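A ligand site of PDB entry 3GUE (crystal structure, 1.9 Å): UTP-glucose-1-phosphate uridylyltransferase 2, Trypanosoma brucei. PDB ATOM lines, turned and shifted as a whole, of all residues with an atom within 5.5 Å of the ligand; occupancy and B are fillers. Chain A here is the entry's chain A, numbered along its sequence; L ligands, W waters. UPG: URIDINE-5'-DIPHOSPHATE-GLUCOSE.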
ATOM      1  N   LEU A  82      -4.535  13.147  18.470  1.00  0.00           N
ATOM      2  CA  LEU A  82      -4.534  13.350  17.021  1.00  0.00           C
ATOM      3  C   LEU A  82      -5.143  12.096  16.333  1.00  0.00           C
ATOM      4  O   LEU A  82      -4.827  10.961  16.686  1.00  0.00           O
ATOM      5  CB  LEU A  82      -3.103  13.612  16.508  1.00  0.00           C
ATOM      6  CG  LEU A  82      -2.319  14.774  17.156  1.00  0.00           C
ATOM      7  CD1 LEU A  82      -0.881  14.901  16.614  1.00  0.00           C
ATOM      8  CD2 LEU A  82      -3.080  16.139  17.065  1.00  0.00           C
ATOM      9  N   ASN A  83      -5.997  12.320  15.338  1.00  0.00           N
ATOM     10  CA  ASN A  83      -6.740  11.218  14.696  1.00  0.00           C
ATOM     11  C   ASN A  83      -7.100  11.524  13.232  1.00  0.00           C
ATOM     12  O   ASN A  83      -8.056  10.973  12.695  1.00  0.00           O
ATOM     13  CB  ASN A  83      -8.000  10.944  15.543  1.00  0.00           C
ATOM     14  CG  ASN A  83      -8.684   9.633  15.167  1.00  0.00           C
ATOM     15  OD1 ASN A  83      -8.049   8.588  15.044  1.00  0.00           O
ATOM     16  ND2 ASN A  83      -9.976   9.714  14.943  1.00  0.00           N
ATOM     17  N   GLY A  84      -6.306  12.393  12.592  1.00  0.00           N
ATOM     18  CA  GLY A  84      -6.661  13.004  11.308  1.00  0.00           C
ATOM     19  C   GLY A  84      -5.897  12.458  10.110  1.00  0.00           C
ATOM     20  O   GLY A  84      -6.272  12.719   8.978  1.00  0.00           O
ATOM     21  N   GLY A  85      -4.863  11.667  10.344  1.00  0.00           N
ATOM     22  CA  GLY A  85      -4.041  11.162   9.239  1.00  0.00           C
ATOM     23  C   GLY A  85      -4.740  10.038   8.494  1.00  0.00           C
ATOM     24  O   GLY A  85      -5.707   9.447   8.993  1.00  0.00           O
ATOM     25  N   LEU A  86      -4.214   9.715   7.322  1.00  0.00           N
ATOM     26  CA  LEU A  86      -4.899   8.840   6.387  1.00  0.00           C
ATOM     27  C   LEU A  86      -4.267   7.462   6.368  1.00  0.00           C
ATOM     28  O   LEU A  86      -4.867   6.517   5.826  1.00  0.00           O
ATOM     29  CB  LEU A  86      -4.895   9.435   4.988  1.00  0.00           C
ATOM     30  CG  LEU A  86      -5.132  10.939   4.872  1.00  0.00           C
ATOM     31  CD1 LEU A  86      -4.744  11.438   3.491  1.00  0.00           C
ATOM     32  CD2 LEU A  86      -6.572  11.278   5.221  1.00  0.00           C
ATOM     33  N   LYS A  96      -6.116   4.907  11.128  1.00  0.00           N
ATOM     34  CA  LYS A  96      -5.261   3.847  11.701  1.00  0.00           C
ATOM     35  C   LYS A  96      -5.670   3.486  13.127  1.00  0.00           C
ATOM     36  O   LYS A  96      -5.414   2.393  13.566  1.00  0.00           O
ATOM     37  CB  LYS A  96      -3.791   4.276  11.664  1.00  0.00           C
ATOM     38  CG  LYS A  96      -2.799   3.230  12.148  1.00  0.00           C
ATOM     39  CD  LYS A  96      -1.443   3.881  12.372  1.00  0.00           C
ATOM     40  CE  LYS A  96      -0.776   4.189  11.032  1.00  0.00           C
ATOM     41  NZ  LYS A  96       0.292   5.234  11.146  1.00  0.00           N
ATOM     42  N   MET A 131      -8.814  15.029  17.179  1.00  0.00           N
ATOM     43  CA  MET A 131      -8.737  15.792  15.967  1.00  0.00           C
ATOM     44  C   MET A 131      -8.910  14.864  14.789  1.00  0.00           C
ATOM     45  O   MET A 131      -8.017  14.042  14.471  1.00  0.00           O
ATOM     46  CB  MET A 131      -7.427  16.560  15.868  1.00  0.00           C
ATOM     47  CG  MET A 131      -7.402  17.554  14.703  1.00  0.00           C
ATOM     48  SD  MET A 131      -6.010  18.679  14.752  1.00  0.00           S
ATOM     49  CE  MET A 131      -4.708  17.718  13.916  1.00  0.00           C
ATOM     50  N   GLN A 162     -10.353  19.127  11.615  1.00  0.00           N
ATOM     51  CA  GLN A 162      -9.303  19.895  11.013  1.00  0.00           C
ATOM     52  C   GLN A 162      -9.692  20.257   9.571  1.00  0.00           C
ATOM     53  O   GLN A 162     -10.790  19.937   9.089  1.00  0.00           O
ATOM     54  CB  GLN A 162      -7.954  19.160  11.107  1.00  0.00           C
ATOM     55  CG  GLN A 162      -7.785  17.931  10.202  1.00  0.00           C
ATOM     56  CD  GLN A 162      -6.364  17.406  10.272  1.00  0.00           C
ATOM     57  OE1 GLN A 162      -6.134  16.273  10.686  1.00  0.00           O
ATOM     58  NE2 GLN A 162      -5.408  18.243   9.921  1.00  0.00           N
ATOM     59  N   PRO A 188      -5.536  16.139   4.588  1.00  0.00           N
ATOM     60  CA  PRO A 188      -5.430  16.974   5.794  1.00  0.00           C
ATOM     61  C   PRO A 188      -4.013  17.577   5.785  1.00  0.00           C
ATOM     62  O   PRO A 188      -3.073  16.875   5.411  1.00  0.00           O
ATOM     63  CB  PRO A 188      -5.583  15.971   6.950  1.00  0.00           C
ATOM     64  CG  PRO A 188      -5.265  14.623   6.362  1.00  0.00           C
ATOM     65  CD  PRO A 188      -5.777  14.726   4.932  1.00  0.00           C
ATOM     66  N   PRO A 189      -3.865  18.855   6.180  1.00  0.00           N
ATOM     67  CA  PRO A 189      -2.562  19.529   5.986  1.00  0.00           C
ATOM     68  C   PRO A 189      -1.470  19.276   7.056  1.00  0.00           C
ATOM     69  O   PRO A 189      -0.588  20.114   7.241  1.00  0.00           O
ATOM     70  CB  PRO A 189      -2.954  21.001   5.955  1.00  0.00           C
ATOM     71  CG  PRO A 189      -4.197  21.099   6.780  1.00  0.00           C
ATOM     72  CD  PRO A 189      -4.878  19.765   6.788  1.00  0.00           C
ATOM     73  N   GLY A 190      -1.549  18.146   7.770  1.00  0.00           N
ATOM     74  CA  GLY A 190      -0.577  17.784   8.825  1.00  0.00           C
ATOM     75  C   GLY A 190      -1.205  18.057  10.172  1.00  0.00           C
ATOM     76  O   GLY A 190      -2.165  18.820  10.247  1.00  0.00           O
ATOM     77  N   HIS A 191      -0.705  17.403  11.221  1.00  0.00           N
ATOM     78  CA  HIS A 191      -1.059  17.710  12.609  1.00  0.00           C
ATOM     79  C   HIS A 191      -0.615  19.128  13.077  1.00  0.00           C
ATOM     80  O   HIS A 191      -1.152  19.660  14.035  1.00  0.00           O
ATOM     81  CB  HIS A 191      -0.650  16.565  13.585  1.00  0.00           C
ATOM     82  CG  HIS A 191       0.742  16.042  13.347  1.00  0.00           C
ATOM     83  ND1 HIS A 191       1.878  16.783  13.600  1.00  0.00           N
ATOM     84  CD2 HIS A 191       1.176  14.871  12.813  1.00  0.00           C
ATOM     85  CE1 HIS A 191       2.952  16.089  13.260  1.00  0.00           C
ATOM     86  NE2 HIS A 191       2.557  14.926  12.771  1.00  0.00           N
ATOM     87  N   SER A 218      -1.033  14.141  21.928  1.00  0.00           N
ATOM     88  CA  SER A 218      -0.248  12.981  21.503  1.00  0.00           C
ATOM     89  C   SER A 218      -0.860  12.278  20.270  1.00  0.00           C
ATOM     90  O   SER A 218      -2.038  12.471  19.950  1.00  0.00           O
ATOM     91  CB  SER A 218      -0.137  11.971  22.656  1.00  0.00           C
ATOM     92  OG  SER A 218      -1.413  11.444  22.989  1.00  0.00           O
ATOM     93  N   ASN A 219      -0.031  11.483  19.603  1.00  0.00           N
ATOM     94  CA  ASN A 219      -0.374  10.707  18.449  1.00  0.00           C
ATOM     95  C   ASN A 219      -1.456   9.683  18.745  1.00  0.00           C
ATOM     96  O   ASN A 219      -1.406   9.007  19.777  1.00  0.00           O
ATOM     97  CB  ASN A 219       0.883  10.006  17.899  1.00  0.00           C
ATOM     98  CG  ASN A 219       1.818  10.951  17.155  1.00  0.00           C
ATOM     99  OD1 ASN A 219       1.461  12.102  16.829  1.00  0.00           O
ATOM    100  ND2 ASN A 219       3.018  10.461  16.837  1.00  0.00           N
ATOM    101  N   GLY A 220      -2.450   9.568  17.867  1.00  0.00           N
ATOM    102  CA  GLY A 220      -3.433   8.472  18.025  1.00  0.00           C
ATOM    103  C   GLY A 220      -2.880   7.047  18.068  1.00  0.00           C
ATOM    104  O   GLY A 220      -3.508   6.144  18.640  1.00  0.00           O
ATOM    105  N   ASP A 221      -1.736   6.838  17.440  1.00  0.00           N
ATOM    106  CA  ASP A 221      -1.038   5.530  17.396  1.00  0.00           C
ATOM    107  C   ASP A 221      -0.159   5.223  18.629  1.00  0.00           C
ATOM    108  O   ASP A 221       0.268   4.078  18.835  1.00  0.00           O
ATOM    109  CB  ASP A 221      -0.185   5.408  16.121  1.00  0.00           C
ATOM    110  CG  ASP A 221       0.927   6.461  16.054  1.00  0.00           C
ATOM    111  OD1 ASP A 221       2.060   6.167  16.468  1.00  0.00           O
ATOM    112  OD2 ASP A 221       0.658   7.586  15.624  1.00  0.00           O
ATOM    113  N   LYS A 255      11.285   6.733  11.238  1.00  0.00           N
ATOM    114  CA  LYS A 255      10.307   7.653  10.657  1.00  0.00           C
ATOM    115  C   LYS A 255       9.676   8.543  11.744  1.00  0.00           C
ATOM    116  O   LYS A 255       9.145   8.070  12.744  1.00  0.00           O
ATOM    117  CB  LYS A 255       9.211   6.855   9.898  1.00  0.00           C
ATOM    118  CG  LYS A 255       9.762   6.101   8.639  1.00  0.00           C
ATOM    119  CD  LYS A 255       8.650   5.263   7.949  1.00  0.00           C
ATOM    120  CE  LYS A 255       7.635   6.107   7.156  1.00  0.00           C
ATOM    121  NZ  LYS A 255       6.397   5.296   6.772  1.00  0.00           N
ATOM    122  N   GLY A 256       9.781   9.851  11.518  1.00  0.00           N
ATOM    123  CA  GLY A 256       9.257  10.860  12.426  1.00  0.00           C
ATOM    124  C   GLY A 256      10.247  12.010  12.399  1.00  0.00           C
ATOM    125  O   GLY A 256      10.792  12.324  11.351  1.00  0.00           O
ATOM    126  N   GLY A 257      10.457  12.658  13.540  1.00  0.00           N
ATOM    127  CA  GLY A 257      11.397  13.763  13.619  1.00  0.00           C
ATOM    128  C   GLY A 257      12.389  13.741  14.772  1.00  0.00           C
ATOM    129  O   GLY A 257      12.059  13.294  15.861  1.00  0.00           O
ATOM    130  N   HIS A 258      13.595  14.199  14.510  1.00  0.00           N
ATOM    131  CA  HIS A 258      14.593  14.444  15.569  1.00  0.00           C
ATOM    132  C   HIS A 258      14.813  15.938  15.748  1.00  0.00           C
ATOM    133  O   HIS A 258      14.587  16.743  14.824  1.00  0.00           O
ATOM    134  CB  HIS A 258      15.931  13.753  15.269  1.00  0.00           C
ATOM    135  CG  HIS A 258      16.671  14.317  14.104  1.00  0.00           C
ATOM    136  ND1 HIS A 258      17.495  15.413  14.205  1.00  0.00           N
ATOM    137  CD2 HIS A 258      16.697  13.950  12.796  1.00  0.00           C
ATOM    138  CE1 HIS A 258      18.015  15.684  13.014  1.00  0.00           C
ATOM    139  NE2 HIS A 258      17.544  14.819  12.144  1.00  0.00           N
ATOM    140  N   LEU A 278      13.057  21.129  14.449  1.00  0.00           N
ATOM    141  CA  LEU A 278      12.557  19.774  14.310  1.00  0.00           C
ATOM    142  C   LEU A 278      12.792  19.400  12.854  1.00  0.00           C
ATOM    143  O   LEU A 278      12.370  20.119  11.933  1.00  0.00           O
ATOM    144  CB  LEU A 278      11.087  19.704  14.715  1.00  0.00           C
ATOM    145  CG  LEU A 278      10.287  18.401  14.550  1.00  0.00           C
ATOM    146  CD1 LEU A 278      10.795  17.329  15.482  1.00  0.00           C
ATOM    147  CD2 LEU A 278       8.782  18.707  14.841  1.00  0.00           C
ATOM    148  N   GLU A 280      11.743  16.643  10.352  1.00  0.00           N
ATOM    149  CA  GLU A 280      10.876  15.501  10.025  1.00  0.00           C
ATOM    150  C   GLU A 280      11.455  14.669   8.882  1.00  0.00           C
ATOM    151  O   GLU A 280      12.309  15.146   8.140  1.00  0.00           O
ATOM    152  CB  GLU A 280       9.480  15.960   9.645  1.00  0.00           C
ATOM    153  CG  GLU A 280       8.680  16.638  10.756  1.00  0.00           C
ATOM    154  CD  GLU A 280       8.264  15.685  11.860  1.00  0.00           C
ATOM    155  OE1 GLU A 280       7.349  14.860  11.679  1.00  0.00           O
ATOM    156  OE2 GLU A 280       8.849  15.790  12.926  1.00  0.00           O
ATOM    157  N   PHE A 301      14.654  11.996  19.918  1.00  0.00           N
ATOM    158  CA  PHE A 301      13.566  11.747  18.972  1.00  0.00           C
ATOM    159  C   PHE A 301      12.249  12.231  19.564  1.00  0.00           C
ATOM    160  O   PHE A 301      11.865  11.822  20.646  1.00  0.00           O
ATOM    161  CB  PHE A 301      13.496  10.230  18.666  1.00  0.00           C
ATOM    162  CG  PHE A 301      12.887   9.883  17.327  1.00  0.00           C
ATOM    163  CD1 PHE A 301      13.613  10.051  16.139  1.00  0.00           C
ATOM    164  CD2 PHE A 301      11.615   9.347  17.243  1.00  0.00           C
ATOM    165  CE1 PHE A 301      13.051   9.718  14.923  1.00  0.00           C
ATOM    166  CE2 PHE A 301      11.049   9.022  16.016  1.00  0.00           C
ATOM    167  CZ  PHE A 301      11.758   9.189  14.862  1.00  0.00           C
ATOM    168  N   ASN A 302      11.562  13.094  18.814  1.00  0.00           N
ATOM    169  CA  ASN A 302      10.247  13.585  19.196  1.00  0.00           C
ATOM    170  C   ASN A 302       9.184  12.465  19.325  1.00  0.00           C
ATOM    171  O   ASN A 302       8.966  11.686  18.376  1.00  0.00           O
ATOM    172  CB  ASN A 302       9.786  14.653  18.199  1.00  0.00           C
ATOM    173  CG  ASN A 302       8.417  15.190  18.499  1.00  0.00           C
ATOM    174  OD1 ASN A 302       7.982  15.256  19.689  1.00  0.00           O
ATOM    175  ND2 ASN A 302       7.698  15.601  17.431  1.00  0.00           N
ATOM    176  N   THR A 303       8.550  12.380  20.503  1.00  0.00           N
ATOM    177  CA  THR A 303       7.478  11.434  20.776  1.00  0.00           C
ATOM    178  C   THR A 303       6.156  11.980  20.227  1.00  0.00           C
ATOM    179  O   THR A 303       5.210  11.227  20.052  1.00  0.00           O
ATOM    180  CB  THR A 303       7.278  11.169  22.272  1.00  0.00           C
ATOM    181  OG1 THR A 303       6.768  12.355  22.900  1.00  0.00           O
ATOM    182  CG2 THR A 303       8.574  10.701  22.997  1.00  0.00           C
ATOM    183  N   ASN A 304       6.109  13.295  19.986  1.00  0.00           N
ATOM    184  CA  ASN A 304       4.874  14.056  19.632  1.00  0.00           C
ATOM    185  C   ASN A 304       3.874  14.134  20.821  1.00  0.00           C
ATOM    186  O   ASN A 304       2.734  14.562  20.658  1.00  0.00           O
ATOM    187  CB  ASN A 304       4.230  13.590  18.291  1.00  0.00           C
ATOM    188  CG  ASN A 304       3.885  14.779  17.328  1.00  0.00           C
ATOM    189  OD1 ASN A 304       4.489  15.857  17.431  1.00  0.00           O
ATOM    190  ND2 ASN A 304       2.901  14.594  16.436  1.00  0.00           N
ATOM    191  N   ALA A 351       3.975  20.256  10.810  1.00  0.00           N
ATOM    192  CA  ALA A 351       4.067  19.363  11.994  1.00  0.00           C
ATOM    193  C   ALA A 351       3.900  20.195  13.288  1.00  0.00           C
ATOM    194  O   ALA A 351       4.515  21.276  13.451  1.00  0.00           O
ATOM    195  CB  ALA A 351       5.375  18.641  11.998  1.00  0.00           C
ATOM    196  N   PHE A 372       6.181   6.084  24.925  1.00  0.00           N
ATOM    197  CA  PHE A 372       6.283   6.181  23.473  1.00  0.00           C
ATOM    198  C   PHE A 372       6.330   4.744  22.880  1.00  0.00           C
ATOM    199  O   PHE A 372       7.337   4.077  22.975  1.00  0.00           O
ATOM    200  CB  PHE A 372       7.540   7.006  23.111  1.00  0.00           C
ATOM    201  CG  PHE A 372       7.760   7.218  21.617  1.00  0.00           C
ATOM    202  CD1 PHE A 372       6.792   7.853  20.837  1.00  0.00           C
ATOM    203  CD2 PHE A 372       8.952   6.834  21.025  1.00  0.00           C
ATOM    204  CE1 PHE A 372       7.001   8.056  19.475  1.00  0.00           C
ATOM    205  CE2 PHE A 372       9.180   7.050  19.654  1.00  0.00           C
ATOM    206  CZ  PHE A 372       8.197   7.659  18.881  1.00  0.00           C
ATOM    207  N   PRO A 374       5.242   3.951  19.312  1.00  0.00           N
ATOM    208  CA  PRO A 374       4.713   4.480  18.052  1.00  0.00           C
ATOM    209  C   PRO A 374       4.349   3.359  17.080  1.00  0.00           C
ATOM    210  O   PRO A 374       5.005   2.286  17.073  1.00  0.00           O
ATOM    211  CB  PRO A 374       5.922   5.242  17.472  1.00  0.00           C
ATOM    212  CG  PRO A 374       7.104   4.434  17.949  1.00  0.00           C
ATOM    213  CD  PRO A 374       6.716   4.098  19.392  1.00  0.00           C
ATOM    214  N   VAL A 375       3.343   3.608  16.258  1.00  0.00           N
ATOM    215  CA  VAL A 375       3.030   2.761  15.098  1.00  0.00           C
ATOM    216  C   VAL A 375       2.894   3.647  13.873  1.00  0.00           C
ATOM    217  O   VAL A 375       1.823   4.245  13.651  1.00  0.00           O
ATOM    218  CB  VAL A 375       1.734   1.918  15.313  1.00  0.00           C
ATOM    219  CG1 VAL A 375       1.376   1.110  14.018  1.00  0.00           C
ATOM    220  CG2 VAL A 375       1.906   0.958  16.556  1.00  0.00           C
ATOM    221  N   LYS A 376       3.994   3.757  13.105  1.00  0.00           N
ATOM    222  CA  LYS A 376       4.055   4.476  11.845  1.00  0.00           C
ATOM    223  C   LYS A 376       3.974   3.489  10.681  1.00  0.00           C
ATOM    224  O   LYS A 376       3.479   3.826   9.593  1.00  0.00           O
ATOM    225  CB  LYS A 376       5.401   5.229  11.695  1.00  0.00           C
ATOM    226  CG  LYS A 376       5.858   5.999  12.890  1.00  0.00           C
ATOM    227  CD  LYS A 376       5.040   7.258  13.055  1.00  0.00           C
ATOM    228  CE  LYS A 376       4.017   7.114  14.143  1.00  0.00           C
ATOM    229  NZ  LYS A 376       3.502   8.466  14.499  1.00  0.00           N
HETATM  230  N1  UPG L   1      -2.446  13.354  11.869  1.00  0.00           N
HETATM  231  C2  UPG L   1      -3.505  14.283  11.948  1.00  0.00           C
HETATM  232  N3  UPG L   1      -3.626  15.185  10.896  1.00  0.00           N
HETATM  233  C4  UPG L   1      -2.776  15.198   9.808  1.00  0.00           C
HETATM  234  C5  UPG L   1      -1.712  14.290   9.750  1.00  0.00           C
HETATM  235  C6  UPG L   1      -1.537  13.361  10.763  1.00  0.00           C
HETATM  236  O2  UPG L   1      -4.337  14.336  12.859  1.00  0.00           O
HETATM  237  O4  UPG L   1      -2.995  16.037   8.931  1.00  0.00           O
HETATM  238  C1C UPG L   1      -2.268  12.357  12.979  1.00  0.00           C
HETATM  239  C2C UPG L   1      -2.062  10.873  12.667  1.00  0.00           C
HETATM  240  O2C UPG L   1      -3.319  10.225  12.424  1.00  0.00           O
HETATM  241  C3C UPG L   1      -1.451  10.409  13.991  1.00  0.00           C
HETATM  242  C4C UPG L   1      -0.550  11.577  14.366  1.00  0.00           C
HETATM  243  O4C UPG L   1      -1.054  12.738  13.651  1.00  0.00           O
HETATM  244  O3C UPG L   1      -2.481  10.312  14.962  1.00  0.00           O
HETATM  245  C5C UPG L   1       0.922  11.346  13.906  1.00  0.00           C
HETATM  246  O5C UPG L   1       1.094  11.345  12.514  1.00  0.00           O
HETATM  247  PA  UPG L   1       2.080  10.293  11.796  1.00  0.00           P
HETATM  248  O1A UPG L   1       1.737   8.968  12.398  1.00  0.00           O
HETATM  249  O2A UPG L   1       2.081  10.446  10.341  1.00  0.00           O
HETATM  250  O3A UPG L   1       3.546  10.735  12.410  1.00  0.00           O
HETATM  251  PB  UPG L   1       4.587  11.818  11.794  1.00  0.00           P
HETATM  252  O1B UPG L   1       3.849  13.077  11.564  1.00  0.00           O
HETATM  253  O2B UPG L   1       5.396  11.222  10.689  1.00  0.00           O
HETATM  254  O3B UPG L   1       5.588  11.921  13.034  1.00  0.00           O
HETATM  255  C1' UPG L   1       5.108  12.472  14.311  1.00  0.00           C
HETATM  256  C2' UPG L   1       5.939  13.698  14.662  1.00  0.00           C
HETATM  257  C3' UPG L   1       7.395  13.264  14.724  1.00  0.00           C
HETATM  258  C4' UPG L   1       7.543  12.188  15.821  1.00  0.00           C
HETATM  259  C5' UPG L   1       6.599  10.994  15.526  1.00  0.00           C
HETATM  260  C6' UPG L   1       6.503  10.095  16.736  1.00  0.00           C
HETATM  261  O2' UPG L   1       5.795  14.735  13.672  1.00  0.00           O
HETATM  262  O3' UPG L   1       8.214  14.396  14.957  1.00  0.00           O
HETATM  263  O4' UPG L   1       8.890  11.739  15.899  1.00  0.00           O
HETATM  264  O5' UPG L   1       5.231  11.403  15.271  1.00  0.00           O
HETATM  265  O6' UPG L   1       5.960   8.828  16.334  1.00  0.00           O
HETATM  266  O   HOH W   1       5.974   8.776  10.154  1.00  0.00           O
HETATM  267  O   HOH W   2       3.774   8.048  17.888  1.00  0.00           O
HETATM  268  O   HOH W   3       7.795   7.479  15.215  1.00  0.00           O
HETATM  269  O   HOH W   4      -2.257   8.212  10.533  1.00  0.00           O
HETATM  270  O   HOH W   5       7.207  12.895   9.962  1.00  0.00           O
HETATM  271  O   HOH W   6       5.552  16.970  15.387  1.00  0.00           O
HETATM  272  O   HOH W   7       4.850  15.174  10.365  1.00  0.00           O
HETATM  273  O   HOH W   8      -0.788   7.055  12.794  1.00  0.00           O
HETATM  274  O   HOH W   9      -3.703   7.876  14.390  1.00  0.00           O
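The backbone NH of Asn 302 sits at hydrogen-bond distance from the backbone carbonyl oxygen of Gly 257 (3.0 Å).
N of Asn 304 lies within hydrogen-bond range of OD1 of Asn 302 (2.7 Å).
The backbone carbonyl oxygen (O) of Met 131 sits at hydrogen-bond distance from the backbone NH (N) of Gly 84 (3.0 Å).
The side-chain amide nitrogen of Asn 219 lies close to the side-chain amino group of Lys 376, 3.1 Å away.
The side-chain amino group (NZ) of Lys 376 is in salt-bridge range of the side-chain carboxylate (OD2) of Asp 221 (3.2 Å).
The side-chain amide nitrogen (ND2) of Asn 304 is in hydrogen-bond range of the side-chain amide oxygen (OD1) of Asn 219, at 2.9 Å.
N of Gly 220 is in hydrogen-bond range of O of Leu 82 (3.0 Å).
OD1 of Asp 221 lies within hydrogen-bond range of N of Val 375, at 2.9 Å.
Water W3 lies within hydrogen-bond range of O6' of the ligand (2.5 Å) and O of Lys 255 (2.9 Å).
Water W5 lies within hydrogen-bond range of O2B of the ligand and OE1 of Glu 280.
Water W7 lies within hydrogen-bond range of O1B of the ligand (2.6 Å), OE1 of Glu 280 (2.8 Å) and NE2 of His 191 (3.3 Å).
Water W2 lies within hydrogen-bond range of ND2 of Asn 219, O6' of the ligand, OD1 of Asp 221 and NZ of Lys 376.
Water W6 lies within hydrogen-bond range of OD1 of Asn 304, O2' of the ligand and ND2 of Asn 302.
Water W8 lies within hydrogen-bond range of the side-chain amino group of Lys 96, an oxygen (O1A) of the ligand and the side-chain carboxylate of Asp 221.
Merely in contact with the ligand: Asn 83 (3.6 Å), Met 131 (3.6 Å), Pro 188 (3.3 Å), Asp 221 (3.7 Å), Gly 256 (3.6 Å), Leu 278 (3.9 Å), Phe 301 (3.5 Å), Thr 303 (3.7 Å), Asn 304 (3.5 Å), Phe 372 (3.4 Å) and Pro 374 (3.8 Å).
Hydrophobic or aromatic side chains that line the ligand: Leu 82, Met 131, Pro 188, His 191, Leu 278, Phe 301, Phe 372 and Pro 374.
Within 4 Å of the ligand: Leu 82, Asn 83, Gly 84, Gly 85, Met 131, Gln 162, Pro 188, Gly 190, His 191, Asn 219, Gly 220, Asp 221, Gly 256, Gly 257, Leu 278, Glu 280, Phe 301, Asn 302, Thr 303, Asn 304, Phe 372, Pro 374 and Lys 376.
O of Asn 302 is in hydrogen-bond range of O4' of the ligand (2.5 Å).
An oxygen (O3') of the ligand sits at hydrogen-bond distance from the side-chain amide nitrogen of Asn 302 (2.8 Å).
The side-chain carboxylate (OE1) of Glu 280 lies within hydrogen-bond range of an oxygen (O2') of the ligand, at 2.5 Å.
O1B of the ligand is in hydrogen-bond range of NE2 of His 191.
OE1 of Gln 162 is in hydrogen-bond range of N3 of the ligand (2.7 Å).
N of Gly 84 lies within hydrogen-bond range of O2 of the ligand (2.8 Å).
O1A of the ligand lies within salt-bridge range of NZ of Lys 376 (2.8 Å).
N of Gly 190 lies within hydrogen-bond range of O4 of the ligand.
O5' of the ligand sits at hydrogen-bond distance from ND2 of Asn 219 (2.9 Å).
N of Gly 85 lies within hydrogen-bond range of O2C of the ligand, 3.0 Å away.
The backbone NH of Gly 257 sits at hydrogen-bond distance from an oxygen (O4') of the ligand, at 3.0 Å.
O of Leu 82 lies within hydrogen-bond range of O3C of the ligand (3.0 Å).
The backbone NH (N) of Gly 220 is in hydrogen-bond range of an oxygen (O3C) of the ligand (3.0 Å).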
